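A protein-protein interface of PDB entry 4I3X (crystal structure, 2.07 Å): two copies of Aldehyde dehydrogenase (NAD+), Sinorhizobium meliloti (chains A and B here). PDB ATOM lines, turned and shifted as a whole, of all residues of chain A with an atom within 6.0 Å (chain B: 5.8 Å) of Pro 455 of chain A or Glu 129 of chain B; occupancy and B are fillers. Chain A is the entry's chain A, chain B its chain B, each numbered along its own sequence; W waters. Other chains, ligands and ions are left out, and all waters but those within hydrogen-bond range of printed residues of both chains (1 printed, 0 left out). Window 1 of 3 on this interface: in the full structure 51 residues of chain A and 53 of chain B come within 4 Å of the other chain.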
ATOM      1  N   GLY A 439      12.167  19.218 -10.805  1.00  0.00           N
ATOM      2  CA  GLY A 439      11.492  20.512 -10.927  1.00  0.00           C
ATOM      3  C   GLY A 439      10.147  20.458 -11.635  1.00  0.00           C
ATOM      4  O   GLY A 439       9.310  21.382 -11.460  1.00  0.00           O
ATOM      5  N   THR A 440       9.957  19.421 -12.460  1.00  0.00           N
ATOM      6  CA  THR A 440       8.805  19.278 -13.283  1.00  0.00           C
ATOM      7  C   THR A 440       8.409  17.815 -13.453  1.00  0.00           C
ATOM      8  O   THR A 440       9.272  16.980 -13.670  1.00  0.00           O
ATOM      9  CB  THR A 440       9.073  19.878 -14.695  1.00  0.00           C
ATOM     10  OG1 THR A 440       9.184  21.304 -14.582  1.00  0.00           O
ATOM     11  CG2 THR A 440       7.859  19.576 -15.741  1.00  0.00           C
ATOM     12  N   MET A 453       7.220  30.488 -21.049  1.00  0.00           N
ATOM     13  CA  MET A 453       6.945  31.281 -19.855  1.00  0.00           C
ATOM     14  C   MET A 453       6.605  30.582 -18.511  1.00  0.00           C
ATOM     15  O   MET A 453       6.362  31.276 -17.515  1.00  0.00           O
ATOM     16  CB  MET A 453       5.778  32.227 -20.165  1.00  0.00           C
ATOM     17  CG  MET A 453       4.425  31.553 -20.159  1.00  0.00           C
ATOM     18  SD  MET A 453       3.403  32.818 -20.964  1.00  0.00           S
ATOM     19  CE  MET A 453       1.817  32.274 -20.305  1.00  0.00           C
ATOM     20  N   SER A 454       6.567  29.250 -18.473  1.00  0.00           N
ATOM     21  CA  SER A 454       6.293  28.566 -17.214  1.00  0.00           C
ATOM     22  C   SER A 454       7.608  28.412 -16.442  1.00  0.00           C
ATOM     23  O   SER A 454       8.678  28.393 -17.027  1.00  0.00           O
ATOM     24  CB  SER A 454       5.626  27.204 -17.465  1.00  0.00           C
ATOM     25  OG  SER A 454       6.396  26.489 -18.387  1.00  0.00           O
ATOM     26  N   PRO A 455       7.534  28.316 -15.114  1.00  0.00           N
ATOM     27  CA  PRO A 455       8.783  28.316 -14.344  1.00  0.00           C
ATOM     28  C   PRO A 455       9.610  27.063 -14.720  1.00  0.00           C
ATOM     29  O   PRO A 455       9.090  25.949 -14.676  1.00  0.00           O
ATOM     30  CB  PRO A 455       8.325  28.173 -12.887  1.00  0.00           C
ATOM     31  CG  PRO A 455       6.867  28.657 -12.914  1.00  0.00           C
ATOM     32  CD  PRO A 455       6.320  28.340 -14.282  1.00  0.00           C
ATOM     33  N   PHE A 456      10.881  27.260 -15.049  1.00  0.00           N
ATOM     34  CA  PHE A 456      11.760  26.163 -15.481  1.00  0.00           C
ATOM     35  C   PHE A 456      13.014  26.128 -14.594  1.00  0.00           C
ATOM     36  O   PHE A 456      13.726  27.171 -14.432  1.00  0.00           O
ATOM     37  CB  PHE A 456      12.129  26.348 -17.002  1.00  0.00           C
ATOM     38  CG  PHE A 456      13.088  25.345 -17.497  1.00  0.00           C
ATOM     39  CD1 PHE A 456      12.730  23.988 -17.564  1.00  0.00           C
ATOM     40  CD2 PHE A 456      14.373  25.707 -17.867  1.00  0.00           C
ATOM     41  CE1 PHE A 456      13.642  23.026 -18.000  1.00  0.00           C
ATOM     42  CE2 PHE A 456      15.285  24.739 -18.323  1.00  0.00           C
ATOM     43  CZ  PHE A 456      14.922  23.400 -18.371  1.00  0.00           C
ATOM     44  N   GLY A 457      13.319  24.956 -14.027  1.00  0.00           N
ATOM     45  CA  GLY A 457      14.595  24.780 -13.342  1.00  0.00           C
ATOM     46  C   GLY A 457      14.595  23.535 -12.473  1.00  0.00           C
ATOM     47  O   GLY A 457      13.533  23.106 -12.029  1.00  0.00           O
ATOM     48  N   LYS A 467      14.408  29.445 -10.581  1.00  0.00           N
ATOM     49  CA  LYS A 467      13.679  29.166 -11.810  1.00  0.00           C
ATOM     50  C   LYS A 467      14.008  30.167 -12.900  1.00  0.00           C
ATOM     51  O   LYS A 467      14.257  31.317 -12.633  1.00  0.00           O
ATOM     52  CB  LYS A 467      12.152  29.218 -11.559  1.00  0.00           C
ATOM     53  CG  LYS A 467      11.690  28.140 -10.580  1.00  0.00           C
ATOM     54  CD  LYS A 467      11.881  26.753 -11.209  1.00  0.00           C
ATOM     55  CE  LYS A 467      11.234  25.686 -10.287  1.00  0.00           C
ATOM     56  NZ  LYS A 467      11.052  24.344 -10.948  1.00  0.00           N
ATOM     57  N   GLU A 468      13.915  29.716 -14.138  1.00  0.00           N
ATOM     58  CA  GLU A 468      14.122  30.513 -15.335  1.00  0.00           C
ATOM     59  C   GLU A 468      12.815  30.406 -16.187  1.00  0.00           C
ATOM     60  O   GLU A 468      11.741  30.020 -15.686  1.00  0.00           O
ATOM     61  CB  GLU A 468      15.231  29.828 -16.163  1.00  0.00           C
ATOM     62  CG  GLU A 468      16.627  30.392 -16.187  1.00  0.00           C
ATOM     63  CD  GLU A 468      17.398  29.842 -17.422  1.00  0.00           C
ATOM     64  OE1 GLU A 468      17.004  28.758 -17.995  1.00  0.00           O
ATOM     65  OE2 GLU A 468      18.349  30.539 -17.886  1.00  0.00           O
ATOM     66  N   GLY A 469      12.920  30.669 -17.493  1.00  0.00           N
ATOM     67  CA  GLY A 469      11.735  30.856 -18.343  1.00  0.00           C
ATOM     68  C   GLY A 469      11.501  32.377 -18.250  1.00  0.00           C
ATOM     69  O   GLY A 469      12.091  33.025 -17.338  1.00  0.00           O
ATOM     70  N   GLU A 472      10.038  34.208 -14.934  1.00  0.00           N
ATOM     71  CA  GLU A 472      10.911  34.167 -13.742  1.00  0.00           C
ATOM     72  C   GLU A 472      12.253  34.875 -13.987  1.00  0.00           C
ATOM     73  O   GLU A 472      12.825  35.447 -13.075  1.00  0.00           O
ATOM     74  CB  GLU A 472      11.157  32.694 -13.268  1.00  0.00           C
ATOM     75  CG  GLU A 472       9.869  32.080 -12.657  1.00  0.00           C
ATOM     76  CD  GLU A 472       9.386  32.821 -11.387  1.00  0.00           C
ATOM     77  OE1 GLU A 472      10.159  33.475 -10.634  1.00  0.00           O
ATOM     78  OE2 GLU A 472       8.196  32.790 -11.140  1.00  0.00           O
ATOM     79  N   LYS A 475      11.817  38.487 -13.310  1.00  0.00           N
ATOM     80  CA  LYS A 475      11.870  38.840 -11.905  1.00  0.00           C
ATOM     81  C   LYS A 475      13.254  38.747 -11.346  1.00  0.00           C
ATOM     82  O   LYS A 475      13.677  39.630 -10.609  1.00  0.00           O
ATOM     83  CB  LYS A 475      10.940  37.941 -11.063  1.00  0.00           C
ATOM     84  CG  LYS A 475       9.456  37.989 -11.422  1.00  0.00           C
ATOM     85  CD  LYS A 475       8.834  37.077 -10.390  1.00  0.00           C
ATOM     86  CE  LYS A 475       7.590  36.395 -10.883  1.00  0.00           C
ATOM     87  NZ  LYS A 475       7.074  35.561  -9.722  1.00  0.00           N
ATOM     88  N   ASP B 127      -0.156  30.251  -3.000  1.00  0.00           N
ATOM     89  CA  ASP B 127       0.117  31.063  -4.242  1.00  0.00           C
ATOM     90  C   ASP B 127       0.314  30.238  -5.559  1.00  0.00           C
ATOM     91  O   ASP B 127       0.789  30.776  -6.566  1.00  0.00           O
ATOM     92  CB  ASP B 127       1.329  32.030  -4.029  1.00  0.00           C
ATOM     93  CG  ASP B 127       2.663  31.281  -3.736  1.00  0.00           C
ATOM     94  OD1 ASP B 127       2.760  30.041  -3.780  1.00  0.00           O
ATOM     95  OD2 ASP B 127       3.669  31.945  -3.465  1.00  0.00           O
ATOM     96  N   GLY B 128      -0.063  28.954  -5.576  1.00  0.00           N
ATOM     97  CA  GLY B 128      -0.026  28.156  -6.815  1.00  0.00           C
ATOM     98  C   GLY B 128      -0.558  28.898  -8.025  1.00  0.00           C
ATOM     99  O   GLY B 128      -1.461  29.714  -7.913  1.00  0.00           O
ATOM    100  N   GLU B 129       0.029  28.669  -9.193  1.00  0.00           N
ATOM    101  CA  GLU B 129      -0.469  29.286 -10.404  1.00  0.00           C
ATOM    102  C   GLU B 129      -0.861  28.237 -11.415  1.00  0.00           C
ATOM    103  O   GLU B 129      -0.370  27.118 -11.384  1.00  0.00           O
ATOM    104  CB  GLU B 129       0.644  30.071 -11.127  1.00  0.00           C
ATOM    105  CG  GLU B 129       1.692  30.726 -10.246  1.00  0.00           C
ATOM    106  CD  GLU B 129       2.813  31.353 -11.124  1.00  0.00           C
ATOM    107  OE1 GLU B 129       3.953  30.711 -11.453  1.00  0.00           O
ATOM    108  OE2 GLU B 129       2.450  32.494 -11.514  1.00  0.00           O
ATOM    109  N   ILE B 130      -1.587  28.659 -12.434  1.00  0.00           N
ATOM    110  CA  ILE B 130      -1.962  27.716 -13.443  1.00  0.00           C
ATOM    111  C   ILE B 130      -1.684  28.350 -14.799  1.00  0.00           C
ATOM    112  O   ILE B 130      -1.979  29.543 -14.961  1.00  0.00           O
ATOM    113  CB  ILE B 130      -3.474  27.408 -13.349  1.00  0.00           C
ATOM    114  CG1 ILE B 130      -3.779  26.904 -11.935  1.00  0.00           C
ATOM    115  CG2 ILE B 130      -3.900  26.358 -14.390  1.00  0.00           C
ATOM    116  CD1 ILE B 130      -5.267  26.571 -11.793  1.00  0.00           C
ATOM    117  N   PHE B 131      -1.114  27.570 -15.749  1.00  0.00           N
ATOM    118  CA  PHE B 131      -0.850  28.072 -17.127  1.00  0.00           C
ATOM    119  C   PHE B 131      -1.597  27.247 -18.108  1.00  0.00           C
ATOM    120  O   PHE B 131      -1.655  26.048 -17.966  1.00  0.00           O
ATOM    121  CB  PHE B 131       0.654  27.990 -17.481  1.00  0.00           C
ATOM    122  CG  PHE B 131       1.515  28.823 -16.591  1.00  0.00           C
ATOM    123  CD1 PHE B 131       1.889  30.140 -16.968  1.00  0.00           C
ATOM    124  CD2 PHE B 131       1.947  28.326 -15.366  1.00  0.00           C
ATOM    125  CE1 PHE B 131       2.690  30.942 -16.115  1.00  0.00           C
ATOM    126  CE2 PHE B 131       2.736  29.121 -14.513  1.00  0.00           C
ATOM    127  CZ  PHE B 131       3.103  30.424 -14.874  1.00  0.00           C
ATOM    128  N   ILE B 144      -0.523  23.584 -16.988  1.00  0.00           N
ATOM    129  CA  ILE B 144       0.594  23.424 -16.078  1.00  0.00           C
ATOM    130  C   ILE B 144       0.203  24.085 -14.756  1.00  0.00           C
ATOM    131  O   ILE B 144      -0.378  25.192 -14.767  1.00  0.00           O
ATOM    132  CB  ILE B 144       1.879  24.103 -16.614  1.00  0.00           C
ATOM    133  CG1 ILE B 144       2.327  23.387 -17.908  1.00  0.00           C
ATOM    134  CG2 ILE B 144       3.024  24.141 -15.550  1.00  0.00           C
ATOM    135  CD1 ILE B 144       3.370  24.177 -18.715  1.00  0.00           C
ATOM    136  N   PHE B 145       0.542  23.418 -13.658  1.00  0.00           N
ATOM    137  CA  PHE B 145       0.230  23.856 -12.280  1.00  0.00           C
ATOM    138  C   PHE B 145       1.505  23.935 -11.496  1.00  0.00           C
ATOM    139  O   PHE B 145       2.471  23.232 -11.817  1.00  0.00           O
ATOM    140  CB  PHE B 145      -0.659  22.782 -11.589  1.00  0.00           C
ATOM    141  CG  PHE B 145      -1.931  22.454 -12.377  1.00  0.00           C
ATOM    142  CD1 PHE B 145      -1.893  21.521 -13.427  1.00  0.00           C
ATOM    143  CD2 PHE B 145      -3.127  23.108 -12.085  1.00  0.00           C
ATOM    144  CE1 PHE B 145      -3.059  21.188 -14.153  1.00  0.00           C
ATOM    145  CE2 PHE B 145      -4.287  22.831 -12.811  1.00  0.00           C
ATOM    146  CZ  PHE B 145      -4.258  21.878 -13.857  1.00  0.00           C
ATOM    147  N   THR B 146       1.534  24.759 -10.468  1.00  0.00           N
ATOM    148  CA  THR B 146       2.735  24.875  -9.645  1.00  0.00           C
ATOM    149  C   THR B 146       2.375  24.468  -8.185  1.00  0.00           C
ATOM    150  O   THR B 146       1.214  24.577  -7.763  1.00  0.00           O
ATOM    151  CB  THR B 146       3.333  26.302  -9.656  1.00  0.00           C
ATOM    152  OG1 THR B 146       2.432  27.183  -9.004  1.00  0.00           O
ATOM    153  CG2 THR B 146       3.474  26.829 -11.169  1.00  0.00           C
ATOM    154  N   VAL B 480       9.782  25.506  -6.046  1.00  0.00           N
ATOM    155  CA  VAL B 480       8.540  25.376  -6.846  1.00  0.00           C
ATOM    156  C   VAL B 480       8.694  24.144  -7.744  1.00  0.00           C
ATOM    157  O   VAL B 480       9.738  24.019  -8.378  1.00  0.00           O
ATOM    158  CB  VAL B 480       8.370  26.615  -7.704  1.00  0.00           C
ATOM    159  CG1 VAL B 480       7.122  26.520  -8.619  1.00  0.00           C
ATOM    160  CG2 VAL B 480       8.264  27.855  -6.786  1.00  0.00           C
ATOM    161  N   THR B 482       6.636  22.128 -10.895  1.00  0.00           N
ATOM    162  CA  THR B 482       5.483  22.203 -11.773  1.00  0.00           C
ATOM    163  C   THR B 482       5.010  20.823 -12.177  1.00  0.00           C
ATOM    164  O   THR B 482       5.785  19.857 -12.143  1.00  0.00           O
ATOM    165  CB  THR B 482       5.750  23.038 -13.038  1.00  0.00           C
ATOM    166  OG1 THR B 482       6.737  22.353 -13.839  1.00  0.00           O
ATOM    167  CG2 THR B 482       6.353  24.387 -12.653  1.00  0.00           C
HETATM  168  O   HOH W   1       6.069  32.258 -12.693  1.00  0.00           O
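The backbone carbonyl oxygen (O) of Gly 439 of chain A lies within hydrogen-bond range of the backbone NH (N) of Thr 482 of chain B, at 2.8 Å. OG1 of Thr 440 of chain A lies within hydrogen-bond range of OG1 of Thr 482 of chain B (2.8 Å). The side-chain amino group (NZ) of Lys 467 of chain A is in hydrogen-bond range of the backbone carbonyl oxygen (O) of Val 480 of chain B, at 2.9 Å.
O of Gly 439 of chain A lies within hydrogen-bond range of NZ of Lys 467 of chain A (3.5 Å). The backbone carbonyl oxygen (O) of Gly 457 of chain A sits at hydrogen-bond distance from the side-chain amino group (NZ) of Lys 467 of chain A, at 3.0 Å. The side-chain hydroxyl (OG1) of Thr 146 of chain B sits at hydrogen-bond distance from the backbone NH (N) of Glu 129 of chain B. The backbone carbonyl oxygen (O) of Ile 144 of chain B sits at hydrogen-bond distance from the backbone NH (N) of Phe 131 of chain B, at 2.7 Å.
CE1 of Phe 131 of chain B touches O of Met 453 of chain A, at 3.9 Å. CD1 of Ile 144 of chain B touches OG of Ser 454 of chain A, at 3.8 Å. Pro 455 of chain A touches Glu 129 of chain B (CG to OE1, 3.9 Å). Pro 455 of chain A touches Phe 131 of chain B. Thr 482 of chain B touches Pro 455 of chain A (CG2 to O, 3.7 Å).
Pro 455 of chain A touches just these residues of chain B: Glu 129 (3.9 Å), Phe 131 (3.7 Å) and Thr 482 (3.7 Å). Printed residues of chain A within 4 Å of Val 480 of chain B: Lys 467 (2.9 Å). Of the printed residues of chain B, Thr 440 of chain A touches Thr 482 (2.8 Å). Of the printed residues of chain A, Phe 131 of chain B touches Met 453 (3.9 Å) and Pro 455 (3.7 Å). Of the printed residues of chain B, Lys 467 of chain A touches Val 480. The nearest residue of chain B that does not touch Pro 455 of chain A is Thr 146 of chain B (4.2 Å). The nearest printed residue of chain B that does not touch Gly 439 of chain A is Val 480 of chain B (4.1 Å).
Of the 12 printed residues of chain A, 6 touch a printed residue of chain B. Of the 10 printed residues of chain B, 5 touch a printed residue of chain A. Hydrophobic or aromatic side chains of chain B within 4 Å of the printed part of chain A: Phe 131, Ile 144 and Val 480.
No position is printed for both chains. Of the 8 pairs that touch across the chains among the printed residues, none has its exchanged pair printed and touching as well.
Water W1 lies within hydrogen-bond range of the side-chain carboxylate of Glu 472 of chain A (2.7 Å) and the side-chain carboxylate of Glu 129 of chain B (2.9 Å).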
